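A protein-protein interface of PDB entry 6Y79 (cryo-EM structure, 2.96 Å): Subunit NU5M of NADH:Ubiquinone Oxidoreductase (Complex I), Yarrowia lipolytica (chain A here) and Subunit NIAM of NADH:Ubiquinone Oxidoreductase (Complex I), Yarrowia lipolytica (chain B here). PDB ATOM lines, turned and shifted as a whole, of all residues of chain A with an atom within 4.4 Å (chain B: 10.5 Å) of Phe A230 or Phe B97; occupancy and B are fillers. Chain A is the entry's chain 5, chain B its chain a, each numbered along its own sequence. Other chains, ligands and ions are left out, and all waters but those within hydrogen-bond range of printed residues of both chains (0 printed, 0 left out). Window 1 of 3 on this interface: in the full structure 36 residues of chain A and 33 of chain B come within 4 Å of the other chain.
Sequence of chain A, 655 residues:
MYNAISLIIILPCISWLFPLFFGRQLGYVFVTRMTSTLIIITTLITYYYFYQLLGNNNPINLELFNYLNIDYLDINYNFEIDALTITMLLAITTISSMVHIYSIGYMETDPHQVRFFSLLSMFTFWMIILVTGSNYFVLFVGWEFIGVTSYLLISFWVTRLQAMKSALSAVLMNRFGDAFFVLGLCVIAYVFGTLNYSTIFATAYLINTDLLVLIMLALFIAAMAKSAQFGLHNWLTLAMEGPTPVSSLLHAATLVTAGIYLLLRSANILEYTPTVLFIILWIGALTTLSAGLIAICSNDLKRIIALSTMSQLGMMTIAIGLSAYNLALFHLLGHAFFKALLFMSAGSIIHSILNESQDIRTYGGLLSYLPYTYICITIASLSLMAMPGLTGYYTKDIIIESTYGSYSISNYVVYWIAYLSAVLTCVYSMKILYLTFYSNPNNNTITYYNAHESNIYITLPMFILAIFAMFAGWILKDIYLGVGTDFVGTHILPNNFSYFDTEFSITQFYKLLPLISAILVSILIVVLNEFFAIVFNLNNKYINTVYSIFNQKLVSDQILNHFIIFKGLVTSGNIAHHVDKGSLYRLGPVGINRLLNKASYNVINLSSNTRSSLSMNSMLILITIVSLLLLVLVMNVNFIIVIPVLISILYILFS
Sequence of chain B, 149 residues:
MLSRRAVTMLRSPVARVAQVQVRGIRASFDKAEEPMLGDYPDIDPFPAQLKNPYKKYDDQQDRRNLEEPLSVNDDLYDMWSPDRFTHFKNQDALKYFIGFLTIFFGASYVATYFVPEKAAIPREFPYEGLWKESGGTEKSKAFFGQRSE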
ATOM      1  N   GLN A 229     -15.156  -3.526 -11.303  1.00  0.00           N
ATOM      2  CA  GLN A 229     -14.051  -2.793 -11.894  1.00  0.00           C
ATOM      3  C   GLN A 229     -14.533  -2.057 -13.146  1.00  0.00           C
ATOM      4  O   GLN A 229     -15.734  -1.940 -13.389  1.00  0.00           O
ATOM      5  CB  GLN A 229     -12.893  -3.740 -12.158  1.00  0.00           C
ATOM      6  CG  GLN A 229     -12.462  -4.504 -10.912  1.00  0.00           C
ATOM      7  CD  GLN A 229     -11.789  -3.631  -9.877  1.00  0.00           C
ATOM      8  OE1 GLN A 229     -10.881  -2.871 -10.185  1.00  0.00           O
ATOM      9  NE2 GLN A 229     -12.233  -3.740  -8.637  1.00  0.00           N
ATOM     10  N   PHE A 230     -13.592  -1.558 -13.963  1.00  0.00           N
ATOM     11  CA  PHE A 230     -13.913  -0.486 -14.909  1.00  0.00           C
ATOM     12  C   PHE A 230     -14.724  -0.982 -16.098  1.00  0.00           C
ATOM     13  O   PHE A 230     -15.531  -0.226 -16.655  1.00  0.00           O
ATOM     14  CB  PHE A 230     -12.647   0.208 -15.421  1.00  0.00           C
ATOM     15  CG  PHE A 230     -12.927   1.310 -16.416  1.00  0.00           C
ATOM     16  CD1 PHE A 230     -13.382   2.546 -15.987  1.00  0.00           C
ATOM     17  CD2 PHE A 230     -12.764   1.102 -17.783  1.00  0.00           C
ATOM     18  CE1 PHE A 230     -13.660   3.553 -16.897  1.00  0.00           C
ATOM     19  CE2 PHE A 230     -13.051   2.103 -18.691  1.00  0.00           C
ATOM     20  CZ  PHE A 230     -13.488   3.331 -18.248  1.00  0.00           C
ATOM     21  N   GLY A 231     -14.515  -2.226 -16.520  1.00  0.00           N
ATOM     22  CA  GLY A 231     -15.332  -2.762 -17.596  1.00  0.00           C
ATOM     23  C   GLY A 231     -16.787  -2.927 -17.189  1.00  0.00           C
ATOM     24  O   GLY A 231     -17.687  -2.900 -18.028  1.00  0.00           O
ATOM     25  N   LEU A 232     -17.038  -3.065 -15.888  1.00  0.00           N
ATOM     26  CA  LEU A 232     -18.294  -3.559 -15.378  1.00  0.00           C
ATOM     27  C   LEU A 232     -18.865  -2.711 -14.240  1.00  0.00           C
ATOM     28  O   LEU A 232     -19.627  -3.197 -13.422  1.00  0.00           O
ATOM     29  CB  LEU A 232     -18.117  -4.988 -14.873  1.00  0.00           C
ATOM     30  CG  LEU A 232     -18.265  -6.249 -15.726  1.00  0.00           C
ATOM     31  CD1 LEU A 232     -19.642  -6.253 -16.336  1.00  0.00           C
ATOM     32  CD2 LEU A 232     -17.185  -6.441 -16.779  1.00  0.00           C
ATOM     33  N   HIS A 233     -18.533  -1.421 -14.176  1.00  0.00           N
ATOM     34  CA  HIS A 233     -18.833  -0.679 -12.953  1.00  0.00           C
ATOM     35  C   HIS A 233     -20.265  -0.159 -12.935  1.00  0.00           C
ATOM     36  O   HIS A 233     -20.764   0.239 -11.878  1.00  0.00           O
ATOM     37  CB  HIS A 233     -17.846   0.469 -12.771  1.00  0.00           C
ATOM     38  CG  HIS A 233     -17.935   1.525 -13.825  1.00  0.00           C
ATOM     39  ND1 HIS A 233     -18.566   2.731 -13.616  1.00  0.00           N
ATOM     40  CD2 HIS A 233     -17.443   1.574 -15.083  1.00  0.00           C
ATOM     41  CE1 HIS A 233     -18.477   3.470 -14.705  1.00  0.00           C
ATOM     42  NE2 HIS A 233     -17.795   2.792 -15.610  1.00  0.00           N
ATOM     43  N   LEU A 286      -6.442   1.278 -12.673  1.00  0.00           N
ATOM     44  CA  LEU A 286      -7.356   2.022 -13.533  1.00  0.00           C
ATOM     45  C   LEU A 286      -8.587   2.490 -12.765  1.00  0.00           C
ATOM     46  O   LEU A 286      -8.995   3.656 -12.873  1.00  0.00           O
ATOM     47  CB  LEU A 286      -7.758   1.152 -14.723  1.00  0.00           C
ATOM     48  CG  LEU A 286      -8.792   1.673 -15.711  1.00  0.00           C
ATOM     49  CD1 LEU A 286      -8.290   2.919 -16.372  1.00  0.00           C
ATOM     50  CD2 LEU A 286      -9.076   0.615 -16.745  1.00  0.00           C
ATOM     51  N   THR A 287      -9.186   1.603 -11.970  1.00  0.00           N
ATOM     52  CA  THR A 287     -10.479   1.940 -11.376  1.00  0.00           C
ATOM     53  C   THR A 287     -10.406   2.905 -10.210  1.00  0.00           C
ATOM     54  O   THR A 287     -11.403   3.597  -9.982  1.00  0.00           O
ATOM     55  CB  THR A 287     -11.218   0.705 -10.894  1.00  0.00           C
ATOM     56  OG1 THR A 287     -10.485   0.093  -9.834  1.00  0.00           O
ATOM     57  CG2 THR A 287     -11.348  -0.227 -11.998  1.00  0.00           C
ATOM     58  N   SER A 290     -10.469   6.157 -12.107  1.00  0.00           N
ATOM     59  CA  SER A 290     -11.725   6.371 -12.815  1.00  0.00           C
ATOM     60  C   SER A 290     -12.867   6.681 -11.853  1.00  0.00           C
ATOM     61  O   SER A 290     -13.631   7.624 -12.080  1.00  0.00           O
ATOM     62  CB  SER A 290     -12.059   5.155 -13.667  1.00  0.00           C
ATOM     63  OG  SER A 290     -13.355   5.293 -14.212  1.00  0.00           O
ATOM     64  N   LEU A 554     -17.780   8.808 -16.881  1.00  0.00           N
ATOM     65  CA  LEU A 554     -16.665   8.607 -17.813  1.00  0.00           C
ATOM     66  C   LEU A 554     -17.162   7.840 -19.018  1.00  0.00           C
ATOM     67  O   LEU A 554     -16.880   6.645 -19.125  1.00  0.00           O
ATOM     68  CB  LEU A 554     -15.474   7.860 -17.200  1.00  0.00           C
ATOM     69  CG  LEU A 554     -14.290   8.616 -16.620  1.00  0.00           C
ATOM     70  CD1 LEU A 554     -13.621   9.460 -17.666  1.00  0.00           C
ATOM     71  CD2 LEU A 554     -14.769   9.463 -15.522  1.00  0.00           C
ATOM     72  N   VAL A 555     -17.848   8.477 -19.962  1.00  0.00           N
ATOM     73  CA  VAL A 555     -19.154   8.178 -20.573  1.00  0.00           C
ATOM     74  C   VAL A 555     -19.611   6.704 -20.753  1.00  0.00           C
ATOM     75  O   VAL A 555     -20.582   6.425 -21.465  1.00  0.00           O
ATOM     76  CB  VAL A 555     -19.144   8.966 -21.906  1.00  0.00           C
ATOM     77  CG1 VAL A 555     -18.350   8.254 -22.973  1.00  0.00           C
ATOM     78  CG2 VAL A 555     -20.535   9.451 -22.368  1.00  0.00           C
ATOM     79  N   SER A 556     -18.934   5.757 -20.092  1.00  0.00           N
ATOM     80  CA  SER A 556     -19.116   4.306 -20.037  1.00  0.00           C
ATOM     81  C   SER A 556     -20.512   3.703 -20.179  1.00  0.00           C
ATOM     82  O   SER A 556     -20.639   2.665 -20.828  1.00  0.00           O
ATOM     83  CB  SER A 556     -18.561   3.809 -18.704  1.00  0.00           C
ATOM     84  OG  SER A 556     -19.389   4.232 -17.631  1.00  0.00           O
ATOM     85  N   ILE A 559     -21.433   4.057 -23.712  1.00  0.00           N
ATOM     86  CA  ILE A 559     -20.604   3.174 -24.523  1.00  0.00           C
ATOM     87  C   ILE A 559     -21.046   1.736 -24.382  1.00  0.00           C
ATOM     88  O   ILE A 559     -20.976   0.959 -25.339  1.00  0.00           O
ATOM     89  CB  ILE A 559     -19.135   3.361 -24.108  1.00  0.00           C
ATOM     90  CG1 ILE A 559     -18.781   4.828 -24.230  1.00  0.00           C
ATOM     91  CG2 ILE A 559     -18.192   2.540 -24.960  1.00  0.00           C
ATOM     92  CD1 ILE A 559     -19.049   5.398 -25.596  1.00  0.00           C
ATOM     93  N   PHE B  88     -24.760  13.588 -25.235  1.00  0.00           N
ATOM     94  CA  PHE B  88     -23.741  13.508 -26.270  1.00  0.00           C
ATOM     95  C   PHE B  88     -24.290  12.746 -27.463  1.00  0.00           C
ATOM     96  O   PHE B  88     -25.162  11.889 -27.318  1.00  0.00           O
ATOM     97  CB  PHE B  88     -22.475  12.804 -25.778  1.00  0.00           C
ATOM     98  CG  PHE B  88     -21.763  13.524 -24.680  1.00  0.00           C
ATOM     99  CD1 PHE B  88     -20.934  14.591 -24.959  1.00  0.00           C
ATOM    100  CD2 PHE B  88     -21.909  13.120 -23.366  1.00  0.00           C
ATOM    101  CE1 PHE B  88     -20.269  15.252 -23.946  1.00  0.00           C
ATOM    102  CE2 PHE B  88     -21.248  13.774 -22.348  1.00  0.00           C
ATOM    103  CZ  PHE B  88     -20.427  14.841 -22.640  1.00  0.00           C
ATOM    104  N   LYS B  89     -23.778  13.061 -28.646  1.00  0.00           N
ATOM    105  CA  LYS B  89     -23.945  12.153 -29.770  1.00  0.00           C
ATOM    106  C   LYS B  89     -23.093  10.917 -29.519  1.00  0.00           C
ATOM    107  O   LYS B  89     -22.071  10.988 -28.833  1.00  0.00           O
ATOM    108  CB  LYS B  89     -23.548  12.835 -31.076  1.00  0.00           C
ATOM    109  CG  LYS B  89     -24.299  14.125 -31.346  1.00  0.00           C
ATOM    110  CD  LYS B  89     -25.756  13.857 -31.676  1.00  0.00           C
ATOM    111  CE  LYS B  89     -26.475  15.133 -32.082  1.00  0.00           C
ATOM    112  NZ  LYS B  89     -27.882  14.890 -32.511  1.00  0.00           N
ATOM    113  N   ASN B  90     -23.523   9.775 -30.063  1.00  0.00           N
ATOM    114  CA  ASN B  90     -22.898   8.505 -29.693  1.00  0.00           C
ATOM    115  C   ASN B  90     -21.493   8.370 -30.276  1.00  0.00           C
ATOM    116  O   ASN B  90     -20.602   7.803 -29.630  1.00  0.00           O
ATOM    117  CB  ASN B  90     -23.790   7.344 -30.129  1.00  0.00           C
ATOM    118  CG  ASN B  90     -25.075   7.255 -29.319  1.00  0.00           C
ATOM    119  OD1 ASN B  90     -25.044   7.022 -28.113  1.00  0.00           O
ATOM    120  ND2 ASN B  90     -26.209   7.436 -29.981  1.00  0.00           N
ATOM    121  N   GLN B  91     -21.268   8.904 -31.478  1.00  0.00           N
ATOM    122  CA  GLN B  91     -19.930   8.878 -32.066  1.00  0.00           C
ATOM    123  C   GLN B  91     -18.982   9.813 -31.312  1.00  0.00           C
ATOM    124  O   GLN B  91     -17.800   9.481 -31.109  1.00  0.00           O
ATOM    125  CB  GLN B  91     -20.022   9.205 -33.568  1.00  0.00           C
ATOM    126  CG  GLN B  91     -20.396  10.654 -33.963  1.00  0.00           C
ATOM    127  CD  GLN B  91     -21.898  10.944 -33.931  1.00  0.00           C
ATOM    128  OE1 GLN B  91     -22.686  10.163 -33.402  1.00  0.00           O
ATOM    129  NE2 GLN B  91     -22.286  12.100 -34.461  1.00  0.00           N
ATOM    130  N   ASP B  92     -19.513  10.948 -30.830  1.00  0.00           N
ATOM    131  CA  ASP B  92     -18.764  11.844 -29.954  1.00  0.00           C
ATOM    132  C   ASP B  92     -18.332  11.123 -28.689  1.00  0.00           C
ATOM    133  O   ASP B  92     -17.160  11.164 -28.308  1.00  0.00           O
ATOM    134  CB  ASP B  92     -19.614  13.062 -29.581  1.00  0.00           C
ATOM    135  CG  ASP B  92     -19.713  14.086 -30.692  1.00  0.00           C
ATOM    136  OD1 ASP B  92     -19.281  13.798 -31.827  1.00  0.00           O
ATOM    137  OD2 ASP B  92     -20.224  15.192 -30.418  1.00  0.00           O
ATOM    138  N   ALA B  93     -19.269  10.420 -28.052  1.00  0.00           N
ATOM    139  CA  ALA B  93     -18.994   9.762 -26.786  1.00  0.00           C
ATOM    140  C   ALA B  93     -18.027   8.592 -26.946  1.00  0.00           C
ATOM    141  O   ALA B  93     -17.217   8.349 -26.050  1.00  0.00           O
ATOM    142  CB  ALA B  93     -20.305   9.296 -26.159  1.00  0.00           C
ATOM    143  N   LEU B  94     -18.073   7.869 -28.071  1.00  0.00           N
ATOM    144  CA  LEU B  94     -17.082   6.820 -28.323  1.00  0.00           C
ATOM    145  C   LEU B  94     -15.696   7.414 -28.506  1.00  0.00           C
ATOM    146  O   LEU B  94     -14.700   6.839 -28.043  1.00  0.00           O
ATOM    147  CB  LEU B  94     -17.475   5.987 -29.545  1.00  0.00           C
ATOM    148  CG  LEU B  94     -16.787   4.620 -29.633  1.00  0.00           C
ATOM    149  CD1 LEU B  94     -16.852   3.847 -28.318  1.00  0.00           C
ATOM    150  CD2 LEU B  94     -17.453   3.798 -30.700  1.00  0.00           C
ATOM    151  N   LYS B  95     -15.627   8.593 -29.154  1.00  0.00           N
ATOM    152  CA  LYS B  95     -14.357   9.311 -29.249  1.00  0.00           C
ATOM    153  C   LYS B  95     -13.840   9.739 -27.876  1.00  0.00           C
ATOM    154  O   LYS B  95     -12.657   9.555 -27.576  1.00  0.00           O
ATOM    155  CB  LYS B  95     -14.514  10.511 -30.166  1.00  0.00           C
ATOM    156  CG  LYS B  95     -13.490  11.626 -29.953  1.00  0.00           C
ATOM    157  CD  LYS B  95     -13.868  12.915 -30.649  1.00  0.00           C
ATOM    158  CE  LYS B  95     -15.178  13.458 -30.123  1.00  0.00           C
ATOM    159  NZ  LYS B  95     -15.516  14.775 -30.713  1.00  0.00           N
ATOM    160  N   TYR B  96     -14.723  10.253 -27.011  1.00  0.00           N
ATOM    161  CA  TYR B  96     -14.305  10.702 -25.677  1.00  0.00           C
ATOM    162  C   TYR B  96     -13.875   9.536 -24.792  1.00  0.00           C
ATOM    163  O   TYR B  96     -12.902   9.649 -24.034  1.00  0.00           O
ATOM    164  CB  TYR B  96     -15.430  11.478 -24.982  1.00  0.00           C
ATOM    165  CG  TYR B  96     -15.744  12.830 -25.574  1.00  0.00           C
ATOM    166  CD1 TYR B  96     -14.759  13.792 -25.722  1.00  0.00           C
ATOM    167  CD2 TYR B  96     -17.036  13.154 -25.949  1.00  0.00           C
ATOM    168  CE1 TYR B  96     -15.052  15.030 -26.259  1.00  0.00           C
ATOM    169  CE2 TYR B  96     -17.338  14.377 -26.495  1.00  0.00           C
ATOM    170  CZ  TYR B  96     -16.346  15.314 -26.644  1.00  0.00           C
ATOM    171  OH  TYR B  96     -16.660  16.541 -27.180  1.00  0.00           O
ATOM    172  N   PHE B  97     -14.578   8.406 -24.889  1.00  0.00           N
ATOM    173  CA  PHE B  97     -14.284   7.242 -24.060  1.00  0.00           C
ATOM    174  C   PHE B  97     -12.963   6.594 -24.453  1.00  0.00           C
ATOM    175  O   PHE B  97     -12.100   6.340 -23.597  1.00  0.00           O
ATOM    176  CB  PHE B  97     -15.433   6.249 -24.186  1.00  0.00           C
ATOM    177  CG  PHE B  97     -15.241   4.977 -23.420  1.00  0.00           C
ATOM    178  CD1 PHE B  97     -15.429   4.943 -22.051  1.00  0.00           C
ATOM    179  CD2 PHE B  97     -14.909   3.802 -24.078  1.00  0.00           C
ATOM    180  CE1 PHE B  97     -15.268   3.769 -21.350  1.00  0.00           C
ATOM    181  CE2 PHE B  97     -14.747   2.626 -23.381  1.00  0.00           C
ATOM    182  CZ  PHE B  97     -14.926   2.611 -22.016  1.00  0.00           C
ATOM    183  N   ILE B  98     -12.790   6.315 -25.752  1.00  0.00           N
ATOM    184  CA  ILE B  98     -11.531   5.756 -26.237  1.00  0.00           C
ATOM    185  C   ILE B  98     -10.406   6.765 -26.063  1.00  0.00           C
ATOM    186  O   ILE B  98      -9.251   6.384 -25.825  1.00  0.00           O
ATOM    187  CB  ILE B  98     -11.703   5.299 -27.702  1.00  0.00           C
ATOM    188  CG1 ILE B  98     -12.825   4.265 -27.811  1.00  0.00           C
ATOM    189  CG2 ILE B  98     -10.444   4.676 -28.249  1.00  0.00           C
ATOM    190  CD1 ILE B  98     -12.636   3.055 -26.959  1.00  0.00           C
ATOM    191  N   GLY B  99     -10.745   8.057 -26.099  1.00  0.00           N
ATOM    192  CA  GLY B  99      -9.817   9.095 -25.711  1.00  0.00           C
ATOM    193  C   GLY B  99      -9.272   8.919 -24.317  1.00  0.00           C
ATOM    194  O   GLY B  99      -8.071   8.750 -24.170  1.00  0.00           O
ATOM    195  N   PHE B 100     -10.148   8.888 -23.299  1.00  0.00           N
ATOM    196  CA  PHE B 100      -9.690   8.791 -21.909  1.00  0.00           C
ATOM    197  C   PHE B 100      -8.931   7.497 -21.651  1.00  0.00           C
ATOM    198  O   PHE B 100      -7.952   7.488 -20.887  1.00  0.00           O
ATOM    199  CB  PHE B 100     -10.857   8.894 -20.932  1.00  0.00           C
ATOM    200  CG  PHE B 100     -10.437   8.776 -19.487  1.00  0.00           C
ATOM    201  CD1 PHE B 100      -9.811   9.838 -18.858  1.00  0.00           C
ATOM    202  CD2 PHE B 100     -10.636   7.603 -18.769  1.00  0.00           C
ATOM    203  CE1 PHE B 100      -9.404   9.744 -17.547  1.00  0.00           C
ATOM    204  CE2 PHE B 100     -10.225   7.501 -17.460  1.00  0.00           C
ATOM    205  CZ  PHE B 100      -9.610   8.576 -16.847  1.00  0.00           C
ATOM    206  N   LEU B 101      -9.346   6.405 -22.301  1.00  0.00           N
ATOM    207  CA  LEU B 101      -8.636   5.141 -22.136  1.00  0.00           C
ATOM    208  C   LEU B 101      -7.216   5.206 -22.704  1.00  0.00           C
ATOM    209  O   LEU B 101      -6.254   4.807 -22.033  1.00  0.00           O
ATOM    210  CB  LEU B 101      -9.439   4.006 -22.766  1.00  0.00           C
ATOM    211  CG  LEU B 101     -10.609   3.516 -21.911  1.00  0.00           C
ATOM    212  CD1 LEU B 101     -11.232   2.304 -22.544  1.00  0.00           C
ATOM    213  CD2 LEU B 101     -10.158   3.189 -20.507  1.00  0.00           C
ATOM    214  N   THR B 102      -7.052   5.730 -23.926  1.00  0.00           N
ATOM    215  CA  THR B 102      -5.699   5.785 -24.476  1.00  0.00           C
ATOM    216  C   THR B 102      -4.879   6.892 -23.820  1.00  0.00           C
ATOM    217  O   THR B 102      -3.649   6.789 -23.771  1.00  0.00           O
ATOM    218  CB  THR B 102      -5.712   5.926 -26.005  1.00  0.00           C
ATOM    219  OG1 THR B 102      -4.404   5.632 -26.511  1.00  0.00           O
ATOM    220  CG2 THR B 102      -6.119   7.334 -26.467  1.00  0.00           C
ATOM    221  N   ILE B 103      -5.542   7.904 -23.237  1.00  0.00           N
ATOM    222  CA  ILE B 103      -4.853   8.888 -22.404  1.00  0.00           C
ATOM    223  C   ILE B 103      -4.208   8.197 -21.214  1.00  0.00           C
ATOM    224  O   ILE B 103      -2.995   8.338 -20.991  1.00  0.00           O
ATOM    225  CB  ILE B 103      -5.816  10.008 -21.932  1.00  0.00           C
ATOM    226  CG1 ILE B 103      -6.189  11.020 -23.021  1.00  0.00           C
ATOM    227  CG2 ILE B 103      -5.250  10.753 -20.740  1.00  0.00           C
ATOM    228  CD1 ILE B 103      -7.406  11.863 -22.598  1.00  0.00           C
ATOM    229  N   PHE B 104      -4.985   7.392 -20.481  1.00  0.00           N
ATOM    230  CA  PHE B 104      -4.461   6.734 -19.287  1.00  0.00           C
ATOM    231  C   PHE B 104      -3.390   5.709 -19.627  1.00  0.00           C
ATOM    232  O   PHE B 104      -2.330   5.696 -19.000  1.00  0.00           O
ATOM    233  CB  PHE B 104      -5.587   6.068 -18.501  1.00  0.00           C
ATOM    234  CG  PHE B 104      -5.137   5.427 -17.227  1.00  0.00           C
ATOM    235  CD1 PHE B 104      -4.874   6.199 -16.111  1.00  0.00           C
ATOM    236  CD2 PHE B 104      -4.974   4.054 -17.144  1.00  0.00           C
ATOM    237  CE1 PHE B 104      -4.460   5.611 -14.939  1.00  0.00           C
ATOM    238  CE2 PHE B 104      -4.560   3.467 -15.975  1.00  0.00           C
ATOM    239  CZ  PHE B 104      -4.305   4.246 -14.873  1.00  0.00           C
ATOM    240  N   PHE B 105      -3.632   4.853 -20.623  1.00  0.00           N
ATOM    241  CA  PHE B 105      -2.651   3.808 -20.904  1.00  0.00           C
ATOM    242  C   PHE B 105      -1.403   4.358 -21.594  1.00  0.00           C
ATOM    243  O   PHE B 105      -0.303   3.835 -21.376  1.00  0.00           O
ATOM    244  CB  PHE B 105      -3.298   2.685 -21.711  1.00  0.00           C
ATOM    245  CG  PHE B 105      -4.258   1.845 -20.907  1.00  0.00           C
ATOM    246  CD1 PHE B 105      -3.799   1.035 -19.878  1.00  0.00           C
ATOM    247  CD2 PHE B 105      -5.620   1.864 -21.177  1.00  0.00           C
ATOM    248  CE1 PHE B 105      -4.683   0.268 -19.134  1.00  0.00           C
ATOM    249  CE2 PHE B 105      -6.505   1.105 -20.438  1.00  0.00           C
ATOM    250  CZ  PHE B 105      -6.036   0.304 -19.416  1.00  0.00           C
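Among the printed residues, merely in contact across the chains: Val A555 with Ala B93 (3.3 Å), Ile A559 with Ala B93 (3.5 Å), Phe A230 with Leu B101 (3.6 Å), Leu A286 with Phe B104 (3.6 Å), Phe A230 with Phe B97 (3.6 Å), Ile A559 with Phe B97 (3.6 Å), Ile A559 with Leu B94 (3.6 Å), Leu A554 with Phe B97 (3.7 Å), Leu A554 with Phe B100 (3.7 Å) and Val A555 with Phe B97 (3.7 Å).
No residue of chain B comes within 4 Å of Gln A229.
No residue of chain B comes within 4 Å of Gly A231.
Of the printed residues of chain B, Leu A286 touches Phe B104.
No residue of chain B comes within 4 Å of Thr A287.
Of chain B, only Ala B93 and Phe B97 come within 4 Å of Val A555.
No residue of chain B comes within 4 Å of Ser A556.
Of chain A, only Phe A230, Leu A554, Val A555 and Ile A559 come within 4 Å of Phe B97.
Gly B99 touches none of the printed residues of chain A.
Of the printed residues of chain A, Phe B100 touches Leu A554.
The nearest residue of chain B that does not touch Phe A230 is Phe B100 (5.2 Å).
The nearest residue of chain A that does not touch Phe B97 is Ser A556 (4.1 Å).
Hydrophobic or aromatic side chains of chain A that line the printed part of chain B: Phe A230, Leu A286, Leu A554, Val A555 and Ile A559.
Of the 18 printed residues of chain B, 6 touch a printed residue of chain A.
Printed residues of chain B that touch a printed residue of chain A: Ala B93, Leu B94, Phe B97, Phe B100, Leu B101 and Phe B104.
Hydrophobic or aromatic side chains of chain B within 4 Å of the printed part of chain A: Ala B93, Leu B94, Phe B97, Phe B100, Leu B101 and Phe B104.
Among the printed residues, 10 pairs touch across the chains.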
